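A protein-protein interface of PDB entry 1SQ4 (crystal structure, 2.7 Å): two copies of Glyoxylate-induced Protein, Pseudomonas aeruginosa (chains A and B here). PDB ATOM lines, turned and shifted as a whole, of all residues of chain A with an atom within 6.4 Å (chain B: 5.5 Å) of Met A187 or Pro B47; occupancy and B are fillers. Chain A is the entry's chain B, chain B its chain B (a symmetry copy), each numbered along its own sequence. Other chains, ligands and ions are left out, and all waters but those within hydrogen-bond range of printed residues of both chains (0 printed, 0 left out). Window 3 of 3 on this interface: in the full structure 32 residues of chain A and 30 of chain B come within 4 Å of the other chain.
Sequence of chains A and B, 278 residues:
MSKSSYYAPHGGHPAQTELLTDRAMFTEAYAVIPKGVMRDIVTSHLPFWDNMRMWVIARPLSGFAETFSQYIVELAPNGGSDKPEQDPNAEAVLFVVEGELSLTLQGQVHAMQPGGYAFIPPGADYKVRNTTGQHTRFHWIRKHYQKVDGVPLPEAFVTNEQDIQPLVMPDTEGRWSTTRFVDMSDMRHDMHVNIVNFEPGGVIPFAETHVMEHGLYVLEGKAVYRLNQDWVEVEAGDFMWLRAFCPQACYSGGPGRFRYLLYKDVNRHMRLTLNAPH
O of Asp A149 touches CE2 of Phe B48, 3.2 Å away.
CZ of Phe B48 touches CG2 of Val A151, at 3.8 Å.
Met A187 touches Leu B46 (SD to C, 3.9 Å).
Pro B47 touches Met A187.
Asn A267 touches His B45.
Pro B47 touches Asn A267.
His B45 touches Arg A268 (O to N, 3.8 Å).
Leu B46 touches Arg A268 (CD2 to C, 3.5 Å).
Pro B47 touches Arg A268.
Leu B46 touches His A269.
Printed residues of chain B that touch a printed residue of chain A: His B45, Leu B46, Pro B47 and Phe B48.
Hydrophobic or aromatic side chains of chain B within 4 Å of the printed part of chain A: His B45, Leu B46, Pro B47 and Phe B48.
Among the printed residues, 10 pairs touch across the chains.
Among the printed residues, no Asp or Glu carboxylate lies within 4 Å of a Lys or Arg side-chain nitrogen of the other chain.
Of the printed residues of chain B, Asp A149 touches Phe B48 (3.2 Å).
Printed residues of chain B within 4 Å of Val A151: Phe B48 (3.8 Å).
Met A187 touches just these residues of chain B: Leu B46 (3.9 Å) and Pro B47 (3.7 Å).
Of the printed residues of chain B, His A269 touches Leu B46 (3.5 Å).
Of the printed residues of chain A, His B45 touches Asn A267 (3.0 Å) and Arg A268 (3.8 Å).
Of chain A, only Met A187 (3.7 Å), Asn A267 (3.3 Å) and Arg A268 (3.8 Å) come within 4 Å of Pro B47.
Of the printed residues of chain A, Phe B48 touches Asp A149 and Val A151.
The nearest residue of chain A that does not touch Pro B47 is Val A151 (4.1 Å).
The nearest printed residue of chain A that does not touch Leu B46 is Asn A267 (4.5 Å).
The side-chain sulfur (SD) of Met A187 lies close to the side-chain amide oxygen (OD1) of Asn A267 (3.8 Å).
The guanidinium group of Arg A268 lies within hydrogen-bond range of the backbone carbonyl oxygen of Met A187.
The backbone carbonyl oxygen (O) of His A189 is in hydrogen-bond range of the side-chain amide nitrogen (ND2) of Asn A267.
OG of Ser B81 sits at hydrogen-bond distance from O of Phe B48, 2.6 Å away.
No position is printed for both chains.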
ATOM      1  N   TYR A 145     -23.296   8.986 -25.723  1.00  0.00           N
ATOM      2  CA  TYR A 145     -22.552  10.062 -25.080  1.00  0.00           C
ATOM      3  C   TYR A 145     -22.982  11.426 -25.579  1.00  0.00           C
ATOM      4  O   TYR A 145     -23.241  11.618 -26.762  1.00  0.00           O
ATOM      5  CB  TYR A 145     -21.054   9.900 -25.313  1.00  0.00           C
ATOM      6  CG  TYR A 145     -20.235  11.008 -24.689  1.00  0.00           C
ATOM      7  CD1 TYR A 145     -19.818  12.112 -25.435  1.00  0.00           C
ATOM      8  CD2 TYR A 145     -19.900  10.965 -23.337  1.00  0.00           C
ATOM      9  CE1 TYR A 145     -19.086  13.144 -24.839  1.00  0.00           C
ATOM     10  CE2 TYR A 145     -19.174  11.986 -22.737  1.00  0.00           C
ATOM     11  CZ  TYR A 145     -18.770  13.068 -23.489  1.00  0.00           C
ATOM     12  OH  TYR A 145     -18.051  14.069 -22.880  1.00  0.00           O
ATOM     13  N   VAL A 148     -19.925  17.986 -25.749  1.00  0.00           N
ATOM     14  CA  VAL A 148     -20.126  19.371 -25.388  1.00  0.00           C
ATOM     15  C   VAL A 148     -18.803  20.107 -25.634  1.00  0.00           C
ATOM     16  O   VAL A 148     -17.719  19.658 -25.224  1.00  0.00           O
ATOM     17  CB  VAL A 148     -20.625  19.493 -23.910  1.00  0.00           C
ATOM     18  CG1 VAL A 148     -19.714  18.721 -22.991  1.00  0.00           C
ATOM     19  CG2 VAL A 148     -20.708  20.958 -23.489  1.00  0.00           C
ATOM     20  N   ASP A 149     -18.913  21.227 -26.346  1.00  0.00           N
ATOM     21  CA  ASP A 149     -17.769  22.058 -26.704  1.00  0.00           C
ATOM     22  C   ASP A 149     -16.887  22.408 -25.517  1.00  0.00           C
ATOM     23  O   ASP A 149     -17.383  22.747 -24.444  1.00  0.00           O
ATOM     24  CB  ASP A 149     -18.248  23.352 -27.376  1.00  0.00           C
ATOM     25  CG  ASP A 149     -18.954  23.108 -28.709  1.00  0.00           C
ATOM     26  OD1 ASP A 149     -19.364  24.106 -29.348  1.00  0.00           O
ATOM     27  OD2 ASP A 149     -19.101  21.932 -29.121  1.00  0.00           O
ATOM     28  N   VAL A 151     -15.318  20.562 -23.667  1.00  0.00           N
ATOM     29  CA  VAL A 151     -15.169  19.403 -22.810  1.00  0.00           C
ATOM     30  C   VAL A 151     -14.762  18.231 -23.687  1.00  0.00           C
ATOM     31  O   VAL A 151     -15.562  17.723 -24.470  1.00  0.00           O
ATOM     32  CB  VAL A 151     -16.488  19.059 -22.091  1.00  0.00           C
ATOM     33  CG1 VAL A 151     -16.282  17.875 -21.168  1.00  0.00           C
ATOM     34  CG2 VAL A 151     -16.984  20.252 -21.323  1.00  0.00           C
ATOM     35  N   PRO A 152     -13.501  17.800 -23.581  1.00  0.00           N
ATOM     36  CA  PRO A 152     -12.996  16.675 -24.373  1.00  0.00           C
ATOM     37  C   PRO A 152     -13.661  15.357 -24.002  1.00  0.00           C
ATOM     38  O   PRO A 152     -14.212  15.226 -22.910  1.00  0.00           O
ATOM     39  CB  PRO A 152     -11.500  16.681 -24.064  1.00  0.00           C
ATOM     40  CG  PRO A 152     -11.439  17.249 -22.668  1.00  0.00           C
ATOM     41  CD  PRO A 152     -12.436  18.382 -22.746  1.00  0.00           C
ATOM     42  N   ASP A 183     -14.232  11.081 -11.053  1.00  0.00           N
ATOM     43  CA  ASP A 183     -14.281  12.256 -10.191  1.00  0.00           C
ATOM     44  C   ASP A 183     -15.595  13.000 -10.396  1.00  0.00           C
ATOM     45  O   ASP A 183     -16.067  13.150 -11.520  1.00  0.00           O
ATOM     46  CB  ASP A 183     -13.116  13.196 -10.502  1.00  0.00           C
ATOM     47  CG  ASP A 183     -13.039  14.375  -9.543  1.00  0.00           C
ATOM     48  OD1 ASP A 183     -12.321  15.353  -9.857  1.00  0.00           O
ATOM     49  OD2 ASP A 183     -13.682  14.332  -8.468  1.00  0.00           O
ATOM     50  N   MET A 184     -16.167  13.472  -9.295  1.00  0.00           N
ATOM     51  CA  MET A 184     -17.422  14.203  -9.327  1.00  0.00           C
ATOM     52  C   MET A 184     -17.347  15.486 -10.120  1.00  0.00           C
ATOM     53  O   MET A 184     -18.366  15.997 -10.583  1.00  0.00           O
ATOM     54  CB  MET A 184     -17.874  14.526  -7.910  1.00  0.00           C
ATOM     55  CG  MET A 184     -18.301  13.312  -7.124  1.00  0.00           C
ATOM     56  SD  MET A 184     -19.724  12.360  -8.025  1.00  0.00           S
ATOM     57  CE  MET A 184     -18.736  10.836  -8.736  1.00  0.00           C
ATOM     58  N   SER A 185     -16.148  16.022 -10.272  1.00  0.00           N
ATOM     59  CA  SER A 185     -15.999  17.260 -11.016  1.00  0.00           C
ATOM     60  C   SER A 185     -15.561  17.018 -12.443  1.00  0.00           C
ATOM     61  O   SER A 185     -15.316  17.959 -13.185  1.00  0.00           O
ATOM     62  CB  SER A 185     -14.992  18.177 -10.318  1.00  0.00           C
ATOM     63  OG  SER A 185     -13.735  17.534 -10.161  1.00  0.00           O
ATOM     64  N   ASP A 186     -15.467  15.759 -12.837  1.00  0.00           N
ATOM     65  CA  ASP A 186     -15.036  15.445 -14.190  1.00  0.00           C
ATOM     66  C   ASP A 186     -16.155  15.654 -15.216  1.00  0.00           C
ATOM     67  O   ASP A 186     -16.907  14.730 -15.528  1.00  0.00           O
ATOM     68  CB  ASP A 186     -14.532  14.002 -14.244  1.00  0.00           C
ATOM     69  CG  ASP A 186     -13.795  13.697 -15.526  1.00  0.00           C
ATOM     70  OD1 ASP A 186     -13.282  12.563 -15.670  1.00  0.00           O
ATOM     71  OD2 ASP A 186     -13.725  14.595 -16.394  1.00  0.00           O
ATOM     72  N   MET A 187     -16.259  16.864 -15.754  1.00  0.00           N
ATOM     73  CA  MET A 187     -17.304  17.146 -16.720  1.00  0.00           C
ATOM     74  C   MET A 187     -17.195  16.356 -18.014  1.00  0.00           C
ATOM     75  O   MET A 187     -18.058  16.459 -18.883  1.00  0.00           O
ATOM     76  CB  MET A 187     -17.346  18.640 -17.031  1.00  0.00           C
ATOM     77  CG  MET A 187     -17.671  19.483 -15.811  1.00  0.00           C
ATOM     78  SD  MET A 187     -19.360  18.974 -14.970  1.00  0.00           S
ATOM     79  CE  MET A 187     -18.697  17.889 -13.517  1.00  0.00           C
ATOM     80  N   ARG A 188     -16.145  15.559 -18.155  1.00  0.00           N
ATOM     81  CA  ARG A 188     -15.997  14.781 -19.378  1.00  0.00           C
ATOM     82  C   ARG A 188     -16.997  13.617 -19.410  1.00  0.00           C
ATOM     83  O   ARG A 188     -17.406  13.168 -20.489  1.00  0.00           O
ATOM     84  CB  ARG A 188     -14.563  14.251 -19.513  1.00  0.00           C
ATOM     85  CG  ARG A 188     -13.471  15.335 -19.607  1.00  0.00           C
ATOM     86  CD  ARG A 188     -12.063  14.717 -19.730  1.00  0.00           C
ATOM     87  NE  ARG A 188     -11.856  13.651 -18.746  1.00  0.00           N
ATOM     88  CZ  ARG A 188     -10.769  12.889 -18.657  1.00  0.00           C
ATOM     89  NH1 ARG A 188      -9.753  13.060 -19.496  1.00  0.00           N
ATOM     90  NH2 ARG A 188     -10.709  11.942 -17.729  1.00  0.00           N
ATOM     91  N   HIS A 189     -17.391  13.139 -18.227  1.00  0.00           N
ATOM     92  CA  HIS A 189     -18.346  12.043 -18.127  1.00  0.00           C
ATOM     93  C   HIS A 189     -19.765  12.540 -18.021  1.00  0.00           C
ATOM     94  O   HIS A 189     -20.036  13.514 -17.333  1.00  0.00           O
ATOM     95  CB  HIS A 189     -18.045  11.151 -16.929  1.00  0.00           C
ATOM     96  CG  HIS A 189     -16.926  10.194 -17.170  1.00  0.00           C
ATOM     97  ND1 HIS A 189     -15.614  10.514 -16.921  1.00  0.00           N
ATOM     98  CD2 HIS A 189     -16.925   8.950 -17.703  1.00  0.00           C
ATOM     99  CE1 HIS A 189     -14.844   9.505 -17.294  1.00  0.00           C
ATOM    100  NE2 HIS A 189     -15.617   8.548 -17.774  1.00  0.00           N
ATOM    101  N   ASP A 190     -20.670  11.851 -18.698  1.00  0.00           N
ATOM    102  CA  ASP A 190     -22.057  12.246 -18.700  1.00  0.00           C
ATOM    103  C   ASP A 190     -22.933  11.171 -18.061  1.00  0.00           C
ATOM    104  O   ASP A 190     -24.161  11.239 -18.115  1.00  0.00           O
ATOM    105  CB  ASP A 190     -22.491  12.511 -20.138  1.00  0.00           C
ATOM    106  CG  ASP A 190     -22.520  11.254 -20.975  1.00  0.00           C
ATOM    107  OD1 ASP A 190     -21.926  10.239 -20.556  1.00  0.00           O
ATOM    108  OD2 ASP A 190     -23.141  11.292 -22.053  1.00  0.00           O
ATOM    109  N   ASN A 267     -24.178  15.675 -15.250  1.00  0.00           N
ATOM    110  CA  ASN A 267     -23.318  16.752 -15.749  1.00  0.00           C
ATOM    111  C   ASN A 267     -23.717  17.372 -17.069  1.00  0.00           C
ATOM    112  O   ASN A 267     -22.874  17.905 -17.795  1.00  0.00           O
ATOM    113  CB  ASN A 267     -21.874  16.277 -15.863  1.00  0.00           C
ATOM    114  CG  ASN A 267     -21.340  15.737 -14.565  1.00  0.00           C
ATOM    115  OD1 ASN A 267     -21.557  16.311 -13.503  1.00  0.00           O
ATOM    116  ND2 ASN A 267     -20.619  14.631 -14.646  1.00  0.00           N
ATOM    117  N   ARG A 268     -25.000  17.324 -17.383  1.00  0.00           N
ATOM    118  CA  ARG A 268     -25.449  17.879 -18.642  1.00  0.00           C
ATOM    119  C   ARG A 268     -26.779  18.609 -18.462  1.00  0.00           C
ATOM    120  O   ARG A 268     -27.423  18.463 -17.431  1.00  0.00           O
ATOM    121  CB  ARG A 268     -25.579  16.743 -19.639  1.00  0.00           C
ATOM    122  CG  ARG A 268     -24.987  17.049 -20.989  1.00  0.00           C
ATOM    123  CD  ARG A 268     -23.630  16.366 -21.256  1.00  0.00           C
ATOM    124  NE  ARG A 268     -22.573  16.748 -20.325  1.00  0.00           N
ATOM    125  CZ  ARG A 268     -21.288  16.434 -20.483  1.00  0.00           C
ATOM    126  NH1 ARG A 268     -20.393  16.811 -19.582  1.00  0.00           N
ATOM    127  NH2 ARG A 268     -20.884  15.755 -21.549  1.00  0.00           N
ATOM    128  N   HIS A 269     -27.183  19.410 -19.441  1.00  0.00           N
ATOM    129  CA  HIS A 269     -28.451  20.121 -19.333  1.00  0.00           C
ATOM    130  C   HIS A 269     -29.579  19.124 -19.517  1.00  0.00           C
ATOM    131  O   HIS A 269     -29.360  18.013 -20.004  1.00  0.00           O
ATOM    132  CB  HIS A 269     -28.569  21.207 -20.410  1.00  0.00           C
ATOM    133  CG  HIS A 269     -28.143  22.565 -19.951  1.00  0.00           C
ATOM    134  ND1 HIS A 269     -28.891  23.323 -19.075  1.00  0.00           N
ATOM    135  CD2 HIS A 269     -27.017  23.276 -20.200  1.00  0.00           C
ATOM    136  CE1 HIS A 269     -28.239  24.442 -18.799  1.00  0.00           C
ATOM    137  NE2 HIS A 269     -27.101  24.435 -19.468  1.00  0.00           N
ATOM    138  N   HIS B  45     -24.699  18.980 -11.580  1.00  0.00           N
ATOM    139  CA  HIS B  45     -23.639  19.890 -11.991  1.00  0.00           C
ATOM    140  C   HIS B  45     -23.622  20.112 -13.500  1.00  0.00           C
ATOM    141  O   HIS B  45     -24.005  19.232 -14.267  1.00  0.00           O
ATOM    142  CB  HIS B  45     -22.284  19.350 -11.504  1.00  0.00           C
ATOM    143  CG  HIS B  45     -22.143  19.337 -10.007  1.00  0.00           C
ATOM    144  ND1 HIS B  45     -21.670  20.420  -9.294  1.00  0.00           N
ATOM    145  CD2 HIS B  45     -22.478  18.399  -9.088  1.00  0.00           C
ATOM    146  CE1 HIS B  45     -21.722  20.150  -8.001  1.00  0.00           C
ATOM    147  NE2 HIS B  45     -22.209  18.932  -7.849  1.00  0.00           N
ATOM    148  N   LEU B  46     -23.210  21.306 -13.919  1.00  0.00           N
ATOM    149  CA  LEU B  46     -23.120  21.643 -15.337  1.00  0.00           C
ATOM    150  C   LEU B  46     -21.692  22.067 -15.638  1.00  0.00           C
ATOM    151  O   LEU B  46     -21.011  22.636 -14.787  1.00  0.00           O
ATOM    152  CB  LEU B  46     -24.073  22.788 -15.700  1.00  0.00           C
ATOM    153  CG  LEU B  46     -25.568  22.490 -15.810  1.00  0.00           C
ATOM    154  CD1 LEU B  46     -26.337  23.800 -15.796  1.00  0.00           C
ATOM    155  CD2 LEU B  46     -25.858  21.705 -17.084  1.00  0.00           C
ATOM    156  N   PRO B  47     -21.217  21.784 -16.859  1.00  0.00           N
ATOM    157  CA  PRO B  47     -19.865  22.129 -17.300  1.00  0.00           C
ATOM    158  C   PRO B  47     -19.621  23.624 -17.231  1.00  0.00           C
ATOM    159  O   PRO B  47     -20.548  24.415 -17.373  1.00  0.00           O
ATOM    160  CB  PRO B  47     -19.841  21.640 -18.744  1.00  0.00           C
ATOM    161  CG  PRO B  47     -20.780  20.512 -18.741  1.00  0.00           C
ATOM    162  CD  PRO B  47     -21.922  21.036 -17.913  1.00  0.00           C
ATOM    163  N   PHE B  48     -18.369  24.000 -17.017  1.00  0.00           N
ATOM    164  CA  PHE B  48     -17.988  25.401 -16.976  1.00  0.00           C
ATOM    165  C   PHE B  48     -18.632  26.251 -15.890  1.00  0.00           C
ATOM    166  O   PHE B  48     -18.938  27.413 -16.127  1.00  0.00           O
ATOM    167  CB  PHE B  48     -18.267  26.052 -18.336  1.00  0.00           C
ATOM    168  CG  PHE B  48     -17.619  25.341 -19.492  1.00  0.00           C
ATOM    169  CD1 PHE B  48     -16.243  25.149 -19.526  1.00  0.00           C
ATOM    170  CD2 PHE B  48     -18.386  24.866 -20.548  1.00  0.00           C
ATOM    171  CE1 PHE B  48     -15.642  24.489 -20.596  1.00  0.00           C
ATOM    172  CE2 PHE B  48     -17.791  24.204 -21.623  1.00  0.00           C
ATOM    173  CZ  PHE B  48     -16.419  24.015 -21.646  1.00  0.00           C
ATOM    174  N   TRP B  49     -18.843  25.687 -14.709  1.00  0.00           N
ATOM    175  CA  TRP B  49     -19.423  26.448 -13.609  1.00  0.00           C
ATOM    176  C   TRP B  49     -18.509  26.333 -12.400  1.00  0.00           C
ATOM    177  O   TRP B  49     -18.004  25.252 -12.105  1.00  0.00           O
ATOM    178  CB  TRP B  49     -20.826  25.938 -13.258  1.00  0.00           C
ATOM    179  CG  TRP B  49     -21.896  26.430 -14.185  1.00  0.00           C
ATOM    180  CD1 TRP B  49     -22.201  25.946 -15.432  1.00  0.00           C
ATOM    181  CD2 TRP B  49     -22.770  27.534 -13.959  1.00  0.00           C
ATOM    182  NE1 TRP B  49     -23.214  26.688 -15.998  1.00  0.00           N
ATOM    183  CE2 TRP B  49     -23.583  27.669 -15.113  1.00  0.00           C
ATOM    184  CE3 TRP B  49     -22.946  28.430 -12.899  1.00  0.00           C
ATOM    185  CZ2 TRP B  49     -24.562  28.661 -15.228  1.00  0.00           C
ATOM    186  CZ3 TRP B  49     -23.917  29.419 -13.013  1.00  0.00           C
ATOM    187  CH2 TRP B  49     -24.714  29.524 -14.169  1.00  0.00           C
ATOM    188  N   SER B  81     -20.441  31.584 -13.678  1.00  0.00           N
ATOM    189  CA  SER B  81     -19.956  31.055 -14.955  1.00  0.00           C
ATOM    190  C   SER B  81     -19.927  32.120 -16.068  1.00  0.00           C
ATOM    191  O   SER B  81     -20.735  33.052 -16.071  1.00  0.00           O
ATOM    192  CB  SER B  81     -20.843  29.877 -15.379  1.00  0.00           C
ATOM    193  OG  SER B  81     -20.539  29.421 -16.683  1.00  0.00           O
ATOM    194  N   LYS B  83     -19.849  31.017 -19.236  1.00  0.00           N
ATOM    195  CA  LYS B  83     -20.403  30.258 -20.339  1.00  0.00           C
ATOM    196  C   LYS B  83     -21.554  29.415 -19.777  1.00  0.00           C
ATOM    197  O   LYS B  83     -21.587  28.193 -19.956  1.00  0.00           O
ATOM    198  CB  LYS B  83     -19.316  29.352 -20.928  1.00  0.00           C
ATOM    199  CG  LYS B  83     -18.043  30.100 -21.348  1.00  0.00           C
ATOM    200  CD  LYS B  83     -16.868  29.160 -21.679  1.00  0.00           C
ATOM    201  CE  LYS B  83     -17.151  28.247 -22.877  1.00  0.00           C
ATOM    202  NZ  LYS B  83     -15.946  27.437 -23.249  1.00  0.00           N
ATOM    203  N   GLN B  86     -25.263  26.650 -22.874  1.00  0.00           N
ATOM    204  CA  GLN B  86     -24.616  26.067 -24.042  1.00  0.00           C
ATOM    205  C   GLN B  86     -25.593  25.976 -25.217  1.00  0.00           C
ATOM    206  O   GLN B  86     -25.212  26.154 -26.369  1.00  0.00           O
ATOM    207  CB  GLN B  86     -24.056  24.676 -23.714  1.00  0.00           C
ATOM    208  CG  GLN B  86     -22.552  24.650 -23.494  1.00  0.00           C
ATOM    209  CD  GLN B  86     -22.119  25.519 -22.321  1.00  0.00           C
ATOM    210  OE1 GLN B  86     -22.387  25.198 -21.156  1.00  0.00           O
ATOM    211  NE2 GLN B  86     -21.452  26.635 -22.624  1.00  0.00           N
